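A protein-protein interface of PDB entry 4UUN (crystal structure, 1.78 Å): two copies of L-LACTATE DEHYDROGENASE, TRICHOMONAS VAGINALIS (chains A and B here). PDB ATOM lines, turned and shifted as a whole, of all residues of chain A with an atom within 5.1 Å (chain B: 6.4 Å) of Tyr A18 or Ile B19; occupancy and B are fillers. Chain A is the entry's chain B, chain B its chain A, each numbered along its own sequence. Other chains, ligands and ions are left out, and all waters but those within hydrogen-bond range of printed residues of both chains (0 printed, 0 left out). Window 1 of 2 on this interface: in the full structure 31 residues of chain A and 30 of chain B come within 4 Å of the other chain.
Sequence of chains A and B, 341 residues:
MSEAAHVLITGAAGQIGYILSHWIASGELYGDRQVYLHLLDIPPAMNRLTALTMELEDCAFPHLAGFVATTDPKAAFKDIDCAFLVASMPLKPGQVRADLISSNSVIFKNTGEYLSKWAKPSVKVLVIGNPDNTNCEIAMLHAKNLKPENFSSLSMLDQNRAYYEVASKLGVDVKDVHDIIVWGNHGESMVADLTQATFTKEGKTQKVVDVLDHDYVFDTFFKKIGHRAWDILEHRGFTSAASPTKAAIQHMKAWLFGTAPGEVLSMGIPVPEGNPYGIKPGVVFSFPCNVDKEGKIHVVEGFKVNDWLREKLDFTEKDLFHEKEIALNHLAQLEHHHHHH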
ATOM      1  N   ALA A  12      13.107 -22.539 -21.493  1.00  0.00           N
ATOM      2  CA  ALA A  12      12.384 -23.732 -21.047  1.00  0.00           C
ATOM      3  C   ALA A  12      12.494 -24.016 -19.551  1.00  0.00           C
ATOM      4  O   ALA A  12      11.633 -24.683 -18.999  1.00  0.00           O
ATOM      5  CB  ALA A  12      12.831 -24.957 -21.846  1.00  0.00           C
ATOM      6  N   GLY A  14      12.368 -21.849 -17.045  1.00  0.00           N
ATOM      7  CA  GLY A  14      11.653 -20.899 -16.210  1.00  0.00           C
ATOM      8  C   GLY A  14      10.298 -21.426 -15.779  1.00  0.00           C
ATOM      9  O   GLY A  14       9.968 -22.573 -16.068  1.00  0.00           O
ATOM     10  N   GLN A  15       9.517 -20.581 -15.105  1.00  0.00           N
ATOM     11  CA  GLN A  15       8.194 -20.951 -14.598  1.00  0.00           C
ATOM     12  C   GLN A  15       7.258 -21.422 -15.702  1.00  0.00           C
ATOM     13  O   GLN A  15       6.599 -22.459 -15.593  1.00  0.00           O
ATOM     14  CB  GLN A  15       7.520 -19.751 -13.934  1.00  0.00           C
ATOM     15  CG  GLN A  15       8.130 -19.264 -12.640  1.00  0.00           C
ATOM     16  CD  GLN A  15       7.310 -18.132 -12.031  1.00  0.00           C
ATOM     17  OE1 GLN A  15       6.802 -18.247 -10.917  1.00  0.00           O
ATOM     18  NE2 GLN A  15       7.167 -17.038 -12.773  1.00  0.00           N
ATOM     19  N   ILE A  16       7.167 -20.623 -16.756  1.00  0.00           N
ATOM     20  CA  ILE A  16       6.255 -20.920 -17.839  1.00  0.00           C
ATOM     21  C   ILE A  16       6.667 -22.201 -18.563  1.00  0.00           C
ATOM     22  O   ILE A  16       5.818 -23.053 -18.847  1.00  0.00           O
ATOM     23  CB  ILE A  16       6.153 -19.718 -18.800  1.00  0.00           C
ATOM     24  CG1 ILE A  16       5.310 -18.612 -18.142  1.00  0.00           C
ATOM     25  CG2 ILE A  16       5.538 -20.122 -20.134  1.00  0.00           C
ATOM     26  CD1 ILE A  16       5.312 -17.280 -18.899  1.00  0.00           C
ATOM     27  N   GLY A  17       7.963 -22.341 -18.844  1.00  0.00           N
ATOM     28  CA  GLY A  17       8.468 -23.518 -19.534  1.00  0.00           C
ATOM     29  C   GLY A  17       8.170 -24.803 -18.779  1.00  0.00           C
ATOM     30  O   GLY A  17       7.846 -25.833 -19.378  1.00  0.00           O
ATOM     31  N   TYR A  18       8.280 -24.734 -17.459  1.00  0.00           N
ATOM     32  CA  TYR A  18       8.088 -25.891 -16.592  1.00  0.00           C
ATOM     33  C   TYR A  18       6.666 -26.422 -16.752  1.00  0.00           C
ATOM     34  O   TYR A  18       6.446 -27.614 -16.977  1.00  0.00           O
ATOM     35  CB  TYR A  18       8.372 -25.466 -15.148  1.00  0.00           C
ATOM     36  CG  TYR A  18       8.193 -26.531 -14.093  1.00  0.00           C
ATOM     37  CD1 TYR A  18       9.162 -27.511 -13.886  1.00  0.00           C
ATOM     38  CD2 TYR A  18       7.079 -26.531 -13.272  1.00  0.00           C
ATOM     39  CE1 TYR A  18       9.005 -28.477 -12.903  1.00  0.00           C
ATOM     40  CE2 TYR A  18       6.910 -27.496 -12.289  1.00  0.00           C
ATOM     41  CZ  TYR A  18       7.878 -28.457 -12.105  1.00  0.00           C
ATOM     42  OH  TYR A  18       7.705 -29.395 -11.118  1.00  0.00           O
ATOM     43  N   ILE A  19       5.699 -25.524 -16.668  1.00  0.00           N
ATOM     44  CA  ILE A  19       4.293 -25.899 -16.796  1.00  0.00           C
ATOM     45  C   ILE A  19       3.945 -26.257 -18.239  1.00  0.00           C
ATOM     46  O   ILE A  19       3.306 -27.275 -18.503  1.00  0.00           O
ATOM     47  CB  ILE A  19       3.371 -24.755 -16.316  1.00  0.00           C
ATOM     48  CG1 ILE A  19       3.686 -24.408 -14.857  1.00  0.00           C
ATOM     49  CG2 ILE A  19       1.908 -25.152 -16.462  1.00  0.00           C
ATOM     50  CD1 ILE A  19       2.990 -23.161 -14.359  1.00  0.00           C
ATOM     51  N   LEU A  20       4.376 -25.411 -19.166  1.00  0.00           N
ATOM     52  CA  LEU A  20       4.073 -25.588 -20.583  1.00  0.00           C
ATOM     53  C   LEU A  20       4.548 -26.955 -21.114  1.00  0.00           C
ATOM     54  O   LEU A  20       3.810 -27.636 -21.825  1.00  0.00           O
ATOM     55  CB  LEU A  20       4.709 -24.439 -21.375  1.00  0.00           C
ATOM     56  CG  LEU A  20       4.449 -24.305 -22.877  1.00  0.00           C
ATOM     57  CD1 LEU A  20       2.963 -24.218 -23.202  1.00  0.00           C
ATOM     58  CD2 LEU A  20       5.191 -23.081 -23.422  1.00  0.00           C
ATOM     59  N   SER A  21       5.774 -27.351 -20.768  1.00  0.00           N
ATOM     60  CA  SER A  21       6.316 -28.626 -21.226  1.00  0.00           C
ATOM     61  C   SER A  21       5.479 -29.811 -20.726  1.00  0.00           C
ATOM     62  O   SER A  21       5.148 -30.710 -21.496  1.00  0.00           O
ATOM     63  CB  SER A  21       7.775 -28.775 -20.782  1.00  0.00           C
ATOM     64  OG  SER A  21       7.898 -28.676 -19.372  1.00  0.00           O
ATOM     65  N   HIS A  22       5.130 -29.806 -19.448  1.00  0.00           N
ATOM     66  CA  HIS A  22       4.314 -30.880 -18.894  1.00  0.00           C
ATOM     67  C   HIS A  22       2.930 -30.948 -19.528  1.00  0.00           C
ATOM     68  O   HIS A  22       2.445 -32.027 -19.871  1.00  0.00           O
ATOM     69  CB  HIS A  22       4.207 -30.738 -17.372  1.00  0.00           C
ATOM     70  CG  HIS A  22       5.422 -31.224 -16.642  1.00  0.00           C
ATOM     71  ND1 HIS A  22       6.506 -30.419 -16.381  1.00  0.00           N
ATOM     72  CD2 HIS A  22       5.725 -32.441 -16.129  1.00  0.00           C
ATOM     73  CE1 HIS A  22       7.429 -31.116 -15.739  1.00  0.00           C
ATOM     74  NE2 HIS A  22       6.979 -32.347 -15.574  1.00  0.00           N
ATOM     75  N   LEU A  52      13.929 -30.233 -14.851  1.00  0.00           N
ATOM     76  CA  LEU A  52      12.690 -30.289 -15.617  1.00  0.00           C
ATOM     77  C   LEU A  52      12.583 -31.598 -16.390  1.00  0.00           C
ATOM     78  O   LEU A  52      11.547 -32.255 -16.361  1.00  0.00           O
ATOM     79  CB  LEU A  52      12.592 -29.104 -16.583  1.00  0.00           C
ATOM     80  CG  LEU A  52      11.573 -29.253 -17.721  1.00  0.00           C
ATOM     81  CD1 LEU A  52      10.168 -29.451 -17.173  1.00  0.00           C
ATOM     82  CD2 LEU A  52      11.623 -28.047 -18.643  1.00  0.00           C
ATOM     83  N   GLU A  55      11.674 -34.570 -14.200  1.00  0.00           N
ATOM     84  CA  GLU A  55      10.254 -34.664 -13.869  1.00  0.00           C
ATOM     85  C   GLU A  55       9.429 -35.072 -15.082  1.00  0.00           C
ATOM     86  O   GLU A  55       8.482 -35.830 -14.937  1.00  0.00           O
ATOM     87  CB  GLU A  55       9.725 -33.362 -13.263  1.00  0.00           C
ATOM     88  CG  GLU A  55      10.160 -33.153 -11.820  1.00  0.00           C
ATOM     89  CD  GLU A  55       9.281 -32.174 -11.091  1.00  0.00           C
ATOM     90  OE1 GLU A  55       8.149 -32.550 -10.719  1.00  0.00           O
ATOM     91  OE2 GLU A  55       9.719 -31.019 -10.893  1.00  0.00           O
ATOM     92  N   ALA B  12      -3.147 -25.707  -0.632  1.00  0.00           N
ATOM     93  CA  ALA B  12      -3.462 -25.204  -1.970  1.00  0.00           C
ATOM     94  C   ALA B  12      -2.498 -24.131  -2.494  1.00  0.00           C
ATOM     95  O   ALA B  12      -2.273 -24.029  -3.704  1.00  0.00           O
ATOM     96  CB  ALA B  12      -4.898 -24.691  -2.005  1.00  0.00           C
ATOM     97  N   GLY B  14       0.676 -23.959  -2.120  1.00  0.00           N
ATOM     98  CA  GLY B  14       2.007 -24.477  -2.416  1.00  0.00           C
ATOM     99  C   GLY B  14       2.207 -24.850  -3.877  1.00  0.00           C
ATOM    100  O   GLY B  14       1.309 -24.676  -4.704  1.00  0.00           O
ATOM    101  N   GLN B  15       3.387 -25.380  -4.196  1.00  0.00           N
ATOM    102  CA  GLN B  15       3.744 -25.696  -5.581  1.00  0.00           C
ATOM    103  C   GLN B  15       2.801 -26.705  -6.231  1.00  0.00           C
ATOM    104  O   GLN B  15       2.329 -26.498  -7.353  1.00  0.00           O
ATOM    105  CB  GLN B  15       5.170 -26.238  -5.652  1.00  0.00           C
ATOM    106  CG  GLN B  15       6.242 -25.205  -5.390  1.00  0.00           C
ATOM    107  CD  GLN B  15       7.605 -25.663  -5.867  1.00  0.00           C
ATOM    108  OE1 GLN B  15       8.315 -24.921  -6.548  1.00  0.00           O
ATOM    109  NE2 GLN B  15       7.978 -26.894  -5.514  1.00  0.00           N
ATOM    110  N   ILE B  16       2.544 -27.807  -5.537  1.00  0.00           N
ATOM    111  CA  ILE B  16       1.660 -28.829  -6.069  1.00  0.00           C
ATOM    112  C   ILE B  16       0.261 -28.248  -6.197  1.00  0.00           C
ATOM    113  O   ILE B  16      -0.378 -28.408  -7.229  1.00  0.00           O
ATOM    114  CB  ILE B  16       1.651 -30.103  -5.191  1.00  0.00           C
ATOM    115  CG1 ILE B  16       2.989 -30.838  -5.349  1.00  0.00           C
ATOM    116  CG2 ILE B  16       0.502 -31.029  -5.593  1.00  0.00           C
ATOM    117  CD1 ILE B  16       3.210 -32.007  -4.390  1.00  0.00           C
ATOM    118  N   GLY B  17      -0.196 -27.560  -5.153  1.00  0.00           N
ATOM    119  CA  GLY B  17      -1.528 -26.976  -5.150  1.00  0.00           C
ATOM    120  C   GLY B  17      -1.753 -26.043  -6.330  1.00  0.00           C
ATOM    121  O   GLY B  17      -2.838 -26.042  -6.933  1.00  0.00           O
ATOM    122  N   TYR B  18      -0.722 -25.263  -6.652  1.00  0.00           N
ATOM    123  CA  TYR B  18      -0.748 -24.285  -7.743  1.00  0.00           C
ATOM    124  C   TYR B  18      -1.045 -24.943  -9.086  1.00  0.00           C
ATOM    125  O   TYR B  18      -1.920 -24.496  -9.830  1.00  0.00           O
ATOM    126  CB  TYR B  18       0.605 -23.576  -7.806  1.00  0.00           C
ATOM    127  CG  TYR B  18       0.754 -22.509  -8.867  1.00  0.00           C
ATOM    128  CD1 TYR B  18       0.199 -21.245  -8.698  1.00  0.00           C
ATOM    129  CD2 TYR B  18       1.479 -22.753 -10.024  1.00  0.00           C
ATOM    130  CE1 TYR B  18       0.353 -20.263  -9.658  1.00  0.00           C
ATOM    131  CE2 TYR B  18       1.637 -21.771 -10.997  1.00  0.00           C
ATOM    132  CZ  TYR B  18       1.069 -20.530 -10.808  1.00  0.00           C
ATOM    133  OH  TYR B  18       1.228 -19.543 -11.760  1.00  0.00           O
ATOM    134  N   ILE B  19      -0.307 -26.006  -9.390  1.00  0.00           N
ATOM    135  CA  ILE B  19      -0.449 -26.716 -10.658  1.00  0.00           C
ATOM    136  C   ILE B  19      -1.702 -27.585 -10.678  1.00  0.00           C
ATOM    137  O   ILE B  19      -2.466 -27.579 -11.652  1.00  0.00           O
ATOM    138  CB  ILE B  19       0.797 -27.590 -10.936  1.00  0.00           C
ATOM    139  CG1 ILE B  19       2.058 -26.722 -11.008  1.00  0.00           C
ATOM    140  CG2 ILE B  19       0.649 -28.354 -12.245  1.00  0.00           C
ATOM    141  CD1 ILE B  19       3.333 -27.505 -10.812  1.00  0.00           C
ATOM    142  N   LEU B  20      -1.916 -28.326  -9.595  1.00  0.00           N
ATOM    143  CA  LEU B  20      -3.086 -29.186  -9.455  1.00  0.00           C
ATOM    144  C   LEU B  20      -4.406 -28.434  -9.650  1.00  0.00           C
ATOM    145  O   LEU B  20      -5.283 -28.901 -10.377  1.00  0.00           O
ATOM    146  CB  LEU B  20      -3.069 -29.844  -8.073  1.00  0.00           C
ATOM    147  CG  LEU B  20      -4.080 -30.947  -7.777  1.00  0.00           C
ATOM    148  CD1 LEU B  20      -4.007 -32.070  -8.797  1.00  0.00           C
ATOM    149  CD2 LEU B  20      -3.850 -31.493  -6.362  1.00  0.00           C
ATOM    150  N   SER B  21      -4.546 -27.278  -9.006  1.00  0.00           N
ATOM    151  CA  SER B  21      -5.774 -26.501  -9.128  1.00  0.00           C
ATOM    152  C   SER B  21      -6.034 -26.105 -10.587  1.00  0.00           C
ATOM    153  O   SER B  21      -7.151 -26.277 -11.087  1.00  0.00           O
ATOM    154  CB  SER B  21      -5.742 -25.276  -8.203  1.00  0.00           C
ATOM    155  OG  SER B  21      -4.636 -24.436  -8.479  1.00  0.00           O
ATOM    156  N   HIS B  22      -5.012 -25.606 -11.277  1.00  0.00           N
ATOM    157  CA  HIS B  22      -5.160 -25.218 -12.673  1.00  0.00           C
ATOM    158  C   HIS B  22      -5.497 -26.402 -13.593  1.00  0.00           C
ATOM    159  O   HIS B  22      -6.359 -26.293 -14.459  1.00  0.00           O
ATOM    160  CB  HIS B  22      -3.887 -24.514 -13.174  1.00  0.00           C
ATOM    161  CG  HIS B  22      -3.802 -23.071 -12.786  1.00  0.00           C
ATOM    162  ND1 HIS B  22      -3.209 -22.646 -11.616  1.00  0.00           N
ATOM    163  CD2 HIS B  22      -4.232 -21.952 -13.415  1.00  0.00           C
ATOM    164  CE1 HIS B  22      -3.283 -21.330 -11.537  1.00  0.00           C
ATOM    165  NE2 HIS B  22      -3.901 -20.882 -12.617  1.00  0.00           N
ATOM    166  N   TRP B  23      -4.807 -27.524 -13.392  1.00  0.00           N
ATOM    167  CA  TRP B  23      -4.997 -28.716 -14.220  1.00  0.00           C
ATOM    168  C   TRP B  23      -6.432 -29.228 -14.079  1.00  0.00           C
ATOM    169  O   TRP B  23      -7.081 -29.579 -15.068  1.00  0.00           O
ATOM    170  CB  TRP B  23      -3.985 -29.807 -13.831  1.00  0.00           C
ATOM    171  CG  TRP B  23      -3.613 -30.753 -14.962  1.00  0.00           C
ATOM    172  CD1 TRP B  23      -4.383 -31.077 -16.042  1.00  0.00           C
ATOM    173  CD2 TRP B  23      -2.379 -31.478 -15.121  1.00  0.00           C
ATOM    174  NE1 TRP B  23      -3.711 -31.958 -16.859  1.00  0.00           N
ATOM    175  CE2 TRP B  23      -2.483 -32.224 -16.314  1.00  0.00           C
ATOM    176  CE3 TRP B  23      -1.204 -31.573 -14.371  1.00  0.00           C
ATOM    177  CZ2 TRP B  23      -1.456 -33.051 -16.773  1.00  0.00           C
ATOM    178  CZ3 TRP B  23      -0.186 -32.396 -14.829  1.00  0.00           C
ATOM    179  CH2 TRP B  23      -0.321 -33.124 -16.018  1.00  0.00           C
ATOM    180  N   ILE B  24      -6.934 -29.242 -12.848  1.00  0.00           N
ATOM    181  CA  ILE B  24      -8.298 -29.691 -12.584  1.00  0.00           C
ATOM    182  C   ILE B  24      -9.288 -28.698 -13.189  1.00  0.00           C
ATOM    183  O   ILE B  24     -10.258 -29.093 -13.847  1.00  0.00           O
ATOM    184  CB  ILE B  24      -8.554 -29.889 -11.080  1.00  0.00           C
ATOM    185  CG1 ILE B  24      -7.757 -31.104 -10.586  1.00  0.00           C
ATOM    186  CG2 ILE B  24     -10.046 -30.077 -10.800  1.00  0.00           C
ATOM    187  CD1 ILE B  24      -7.687 -31.248  -9.077  1.00  0.00           C
ATOM    188  N   LEU B  52      -3.075 -17.224  -6.197  1.00  0.00           N
ATOM    189  CA  LEU B  52      -3.548 -18.394  -6.922  1.00  0.00           C
ATOM    190  C   LEU B  52      -4.952 -18.190  -7.488  1.00  0.00           C
ATOM    191  O   LEU B  52      -5.207 -18.510  -8.650  1.00  0.00           O
ATOM    192  CB  LEU B  52      -3.529 -19.627  -6.014  1.00  0.00           C
ATOM    193  CG  LEU B  52      -4.286 -20.846  -6.557  1.00  0.00           C
ATOM    194  CD1 LEU B  52      -3.726 -21.275  -7.900  1.00  0.00           C
ATOM    195  CD2 LEU B  52      -4.225 -21.988  -5.553  1.00  0.00           C
ATOM    196  N   ARG B 236      16.801 -28.553  -8.964  1.00  0.00           N
ATOM    197  CA  ARG B 236      15.689 -27.607  -9.091  1.00  0.00           C
ATOM    198  C   ARG B 236      15.722 -26.510  -8.030  1.00  0.00           C
ATOM    199  O   ARG B 236      15.244 -25.397  -8.265  1.00  0.00           O
ATOM    200  CB  ARG B 236      14.356 -28.372  -9.019  1.00  0.00           C
ATOM    201  CG  ARG B 236      13.085 -27.521  -8.899  1.00  0.00           C
ATOM    202  CD  ARG B 236      11.843 -28.416  -9.014  1.00  0.00           C
ATOM    203  NE  ARG B 236      10.589 -27.777  -8.602  1.00  0.00           N
ATOM    204  CZ  ARG B 236       9.881 -26.942  -9.358  1.00  0.00           C
ATOM    205  NH1 ARG B 236      10.300 -26.607 -10.568  1.00  0.00           N
ATOM    206  NH2 ARG B 236       8.756 -26.424  -8.894  1.00  0.00           N
ATOM    207  N   THR B 239      11.503 -29.090  -4.309  1.00  0.00           N
ATOM    208  CA  THR B 239      11.045 -30.464  -4.479  1.00  0.00           C
ATOM    209  C   THR B 239      10.171 -30.590  -5.725  1.00  0.00           C
ATOM    210  O   THR B 239       9.693 -29.589  -6.257  1.00  0.00           O
ATOM    211  CB  THR B 239      10.235 -30.914  -3.258  1.00  0.00           C
ATOM    212  OG1 THR B 239       9.267 -29.907  -2.938  1.00  0.00           O
ATOM    213  CG2 THR B 239      11.149 -31.118  -2.059  1.00  0.00           C
ATOM    214  N   SER B 240       9.973 -31.824  -6.186  1.00  0.00           N
ATOM    215  CA  SER B 240       9.147 -32.078  -7.358  1.00  0.00           C
ATOM    216  C   SER B 240       7.744 -31.498  -7.165  1.00  0.00           C
ATOM    217  O   SER B 240       7.265 -31.361  -6.042  1.00  0.00           O
ATOM    218  CB  SER B 240       9.071 -33.580  -7.635  1.00  0.00           C
ATOM    219  OG  SER B 240      10.367 -34.148  -7.739  1.00  0.00           O
ATOM    220  N   ALA B 241       7.094 -31.146  -8.267  1.00  0.00           N
ATOM    221  CA  ALA B 241       5.762 -30.562  -8.202  1.00  0.00           C
ATOM    222  C   ALA B 241       4.895 -31.037  -9.368  1.00  0.00           C
ATOM    223  O   ALA B 241       3.807 -31.573  -9.167  1.00  0.00           O
ATOM    224  CB  ALA B 241       5.858 -29.046  -8.182  1.00  0.00           C
ATOM    225  N   ALA B 242       5.382 -30.854 -10.589  1.00  0.00           N
ATOM    226  CA  ALA B 242       4.625 -31.260 -11.765  1.00  0.00           C
ATOM    227  C   ALA B 242       4.404 -32.775 -11.824  1.00  0.00           C
ATOM    228  O   ALA B 242       3.312 -33.237 -12.167  1.00  0.00           O
ATOM    229  CB  ALA B 242       5.321 -30.767 -13.031  1.00  0.00           C
ATOM    230  N   SER B 243       5.432 -33.548 -11.486  1.00  0.00           N
ATOM    231  CA  SER B 243       5.345 -34.997 -11.611  1.00  0.00           C
ATOM    232  C   SER B 243       4.422 -35.631 -10.559  1.00  0.00           C
ATOM    233  O   SER B 243       3.652 -36.510 -10.910  1.00  0.00           O
ATOM    234  CB  SER B 243       6.737 -35.663 -11.648  1.00  0.00           C
ATOM    235  OG  SER B 243       7.562 -35.283 -10.559  1.00  0.00           O
ATOM    236  N   PRO B 244       4.471 -35.177  -9.284  1.00  0.00           N
ATOM    237  CA  PRO B 244       3.458 -35.727  -8.369  1.00  0.00           C
ATOM    238  C   PRO B 244       2.037 -35.267  -8.696  1.00  0.00           C
ATOM    239  O   PRO B 244       1.095 -36.016  -8.477  1.00  0.00           O
ATOM    240  CB  PRO B 244       3.890 -35.208  -6.991  1.00  0.00           C
ATOM    241  CG  PRO B 244       4.879 -34.136  -7.242  1.00  0.00           C
ATOM    242  CD  PRO B 244       5.522 -34.442  -8.551  1.00  0.00           C
ATOM    243  N   THR B 245       1.887 -34.055  -9.222  1.00  0.00           N
ATOM    244  CA  THR B 245       0.580 -33.586  -9.657  1.00  0.00           C
ATOM    245  C   THR B 245       0.052 -34.496 -10.759  1.00  0.00           C
ATOM    246  O   THR B 245      -1.111 -34.894 -10.732  1.00  0.00           O
ATOM    247  CB  THR B 245       0.625 -32.112 -10.138  1.00  0.00           C
ATOM    248  OG1 THR B 245       1.038 -31.262  -9.057  1.00  0.00           O
ATOM    249  CG2 THR B 245      -0.738 -31.662 -10.618  1.00  0.00           C
ATOM    250  N   ILE B 249      -3.514 -36.702 -10.409  1.00  0.00           N
ATOM    251  CA  ILE B 249      -4.647 -36.616 -11.328  1.00  0.00           C
ATOM    252  C   ILE B 249      -4.916 -37.973 -11.991  1.00  0.00           C
ATOM    253  O   ILE B 249      -6.071 -38.374 -12.163  1.00  0.00           O
ATOM    254  CB  ILE B 249      -4.411 -35.511 -12.385  1.00  0.00           C
ATOM    255  CG1 ILE B 249      -4.454 -34.148 -11.705  1.00  0.00           C
ATOM    256  CG2 ILE B 249      -5.473 -35.548 -13.486  1.00  0.00           C
ATOM    257  CD1 ILE B 249      -3.847 -33.029 -12.524  1.00  0.00           C
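The side-chain amide oxygen of Gln B15 sits at hydrogen-bond distance from the guanidinium group of Arg B236 (2.8 Å).
A ring nitrogen (ND1) of His B22 sits at hydrogen-bond distance from the backbone carbonyl oxygen (O) of Tyr B18, at 2.9 Å.
The backbone carbonyl oxygen (O) of Thr B239 sits at hydrogen-bond distance from the guanidinium group (NE) of Arg B236, 3.1 Å away.
The side-chain hydroxyl (OG1) of Thr B245 is in hydrogen-bond range of the backbone carbonyl oxygen (O) of Ala B241 (2.8 Å).
The backbone carbonyl oxygen (O) of Tyr A18 sits at hydrogen-bond distance from the side-chain hydroxyl (OG) of Ser A21, 3.0 Å away.
O of Tyr A18 sits at hydrogen-bond distance from ND1 of His A22 (2.9 Å).
The side-chain hydroxyl (OH) of Tyr A18 lies within hydrogen-bond range of the backbone NH (N) of Ala B241, 3.4 Å away.
N of Ala B241 sits at hydrogen-bond distance from OE1 of Glu A55 (3.0 Å).
The backbone NH (N) of Ala B242 sits at hydrogen-bond distance from the side-chain hydroxyl (OH) of Tyr A18 (2.8 Å).
The backbone NH (N) of Ala B242 is in hydrogen-bond range of the side-chain carboxylate (OE1) of Glu A55 (3.2 Å).
The side-chain hydroxyl (OG) of Ser B243 sits at hydrogen-bond distance from the side-chain carboxylate (OE1) of Glu A55 (2.8 Å).
Among the printed residues, merely in contact across the chains: Tyr A18 with Ile B19, Tyr A18 with Arg B236, Ile A19 with Tyr B18, His A22 with Ala B242, Glu A55 with Arg B236, Glu A55 with Ser B240 and Glu A55 with Pro B244.
Of the 12 printed residues of chain A, 4 touch a printed residue of chain B.
Printed residues of chain A that touch a printed residue of chain B: Tyr A18, Ile A19, His A22 and Glu A55.
Hydrophobic or aromatic side chains of chain A that line the printed part of chain B: Tyr A18, Ile A19 and His A22.
Printed residues of chain B that touch a printed residue of chain A: Tyr B18, Ile B19, Arg B236, Ser B240, Ala B241, Ala B242, Ser B243 and Pro B244.
Hydrophobic or aromatic side chains of chain B within 4 Å of the printed part of chain A: Tyr B18, Ile B19, Ala B241, Ala B242 and Pro B244.
Along chain B the printed residues that touch a printed residue of chain A span positions 18 to 244.
Among the printed residues, 12 pairs touch across the chains.
Among the printed residues, no Asp or Glu carboxylate lies within 4 Å of a Lys or Arg side-chain nitrogen of the other chain.
Tyr A18 touches Ile B19, and with the chains exchanged Ile A19 touches Tyr B18.
Positions printed for both chains: 12, 14, 15, 16, 17, 18, 19, 20, 21, 22 and 52.
Of the 12 pairs that touch across the chains among the printed residues, 2 have their exchanged pair printed and touching as well.
Of chain B, only Ile B19, Arg B236, Ala B241 and Ala B242 come within 4 Å of Tyr A18.
Of the printed residues of chain B, Glu A55 touches Arg B236, Ser B240, Ala B241, Ala B242, Ser B243 and Pro B244.
Of the printed residues of chain A, Ile B19 touches Tyr A18 (3.9 Å).
Printed residues of chain A within 4 Å of Ala B242: Tyr A18 (2.8 Å), His A22 (3.4 Å) and Glu A55 (3.2 Å).
The nearest printed residue of chain A that does not touch Ile B19 is Ile A19 (4.8 Å).
The nearest printed residue of chain B that does not touch Glu A55 is Thr B239 (4.9 Å).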
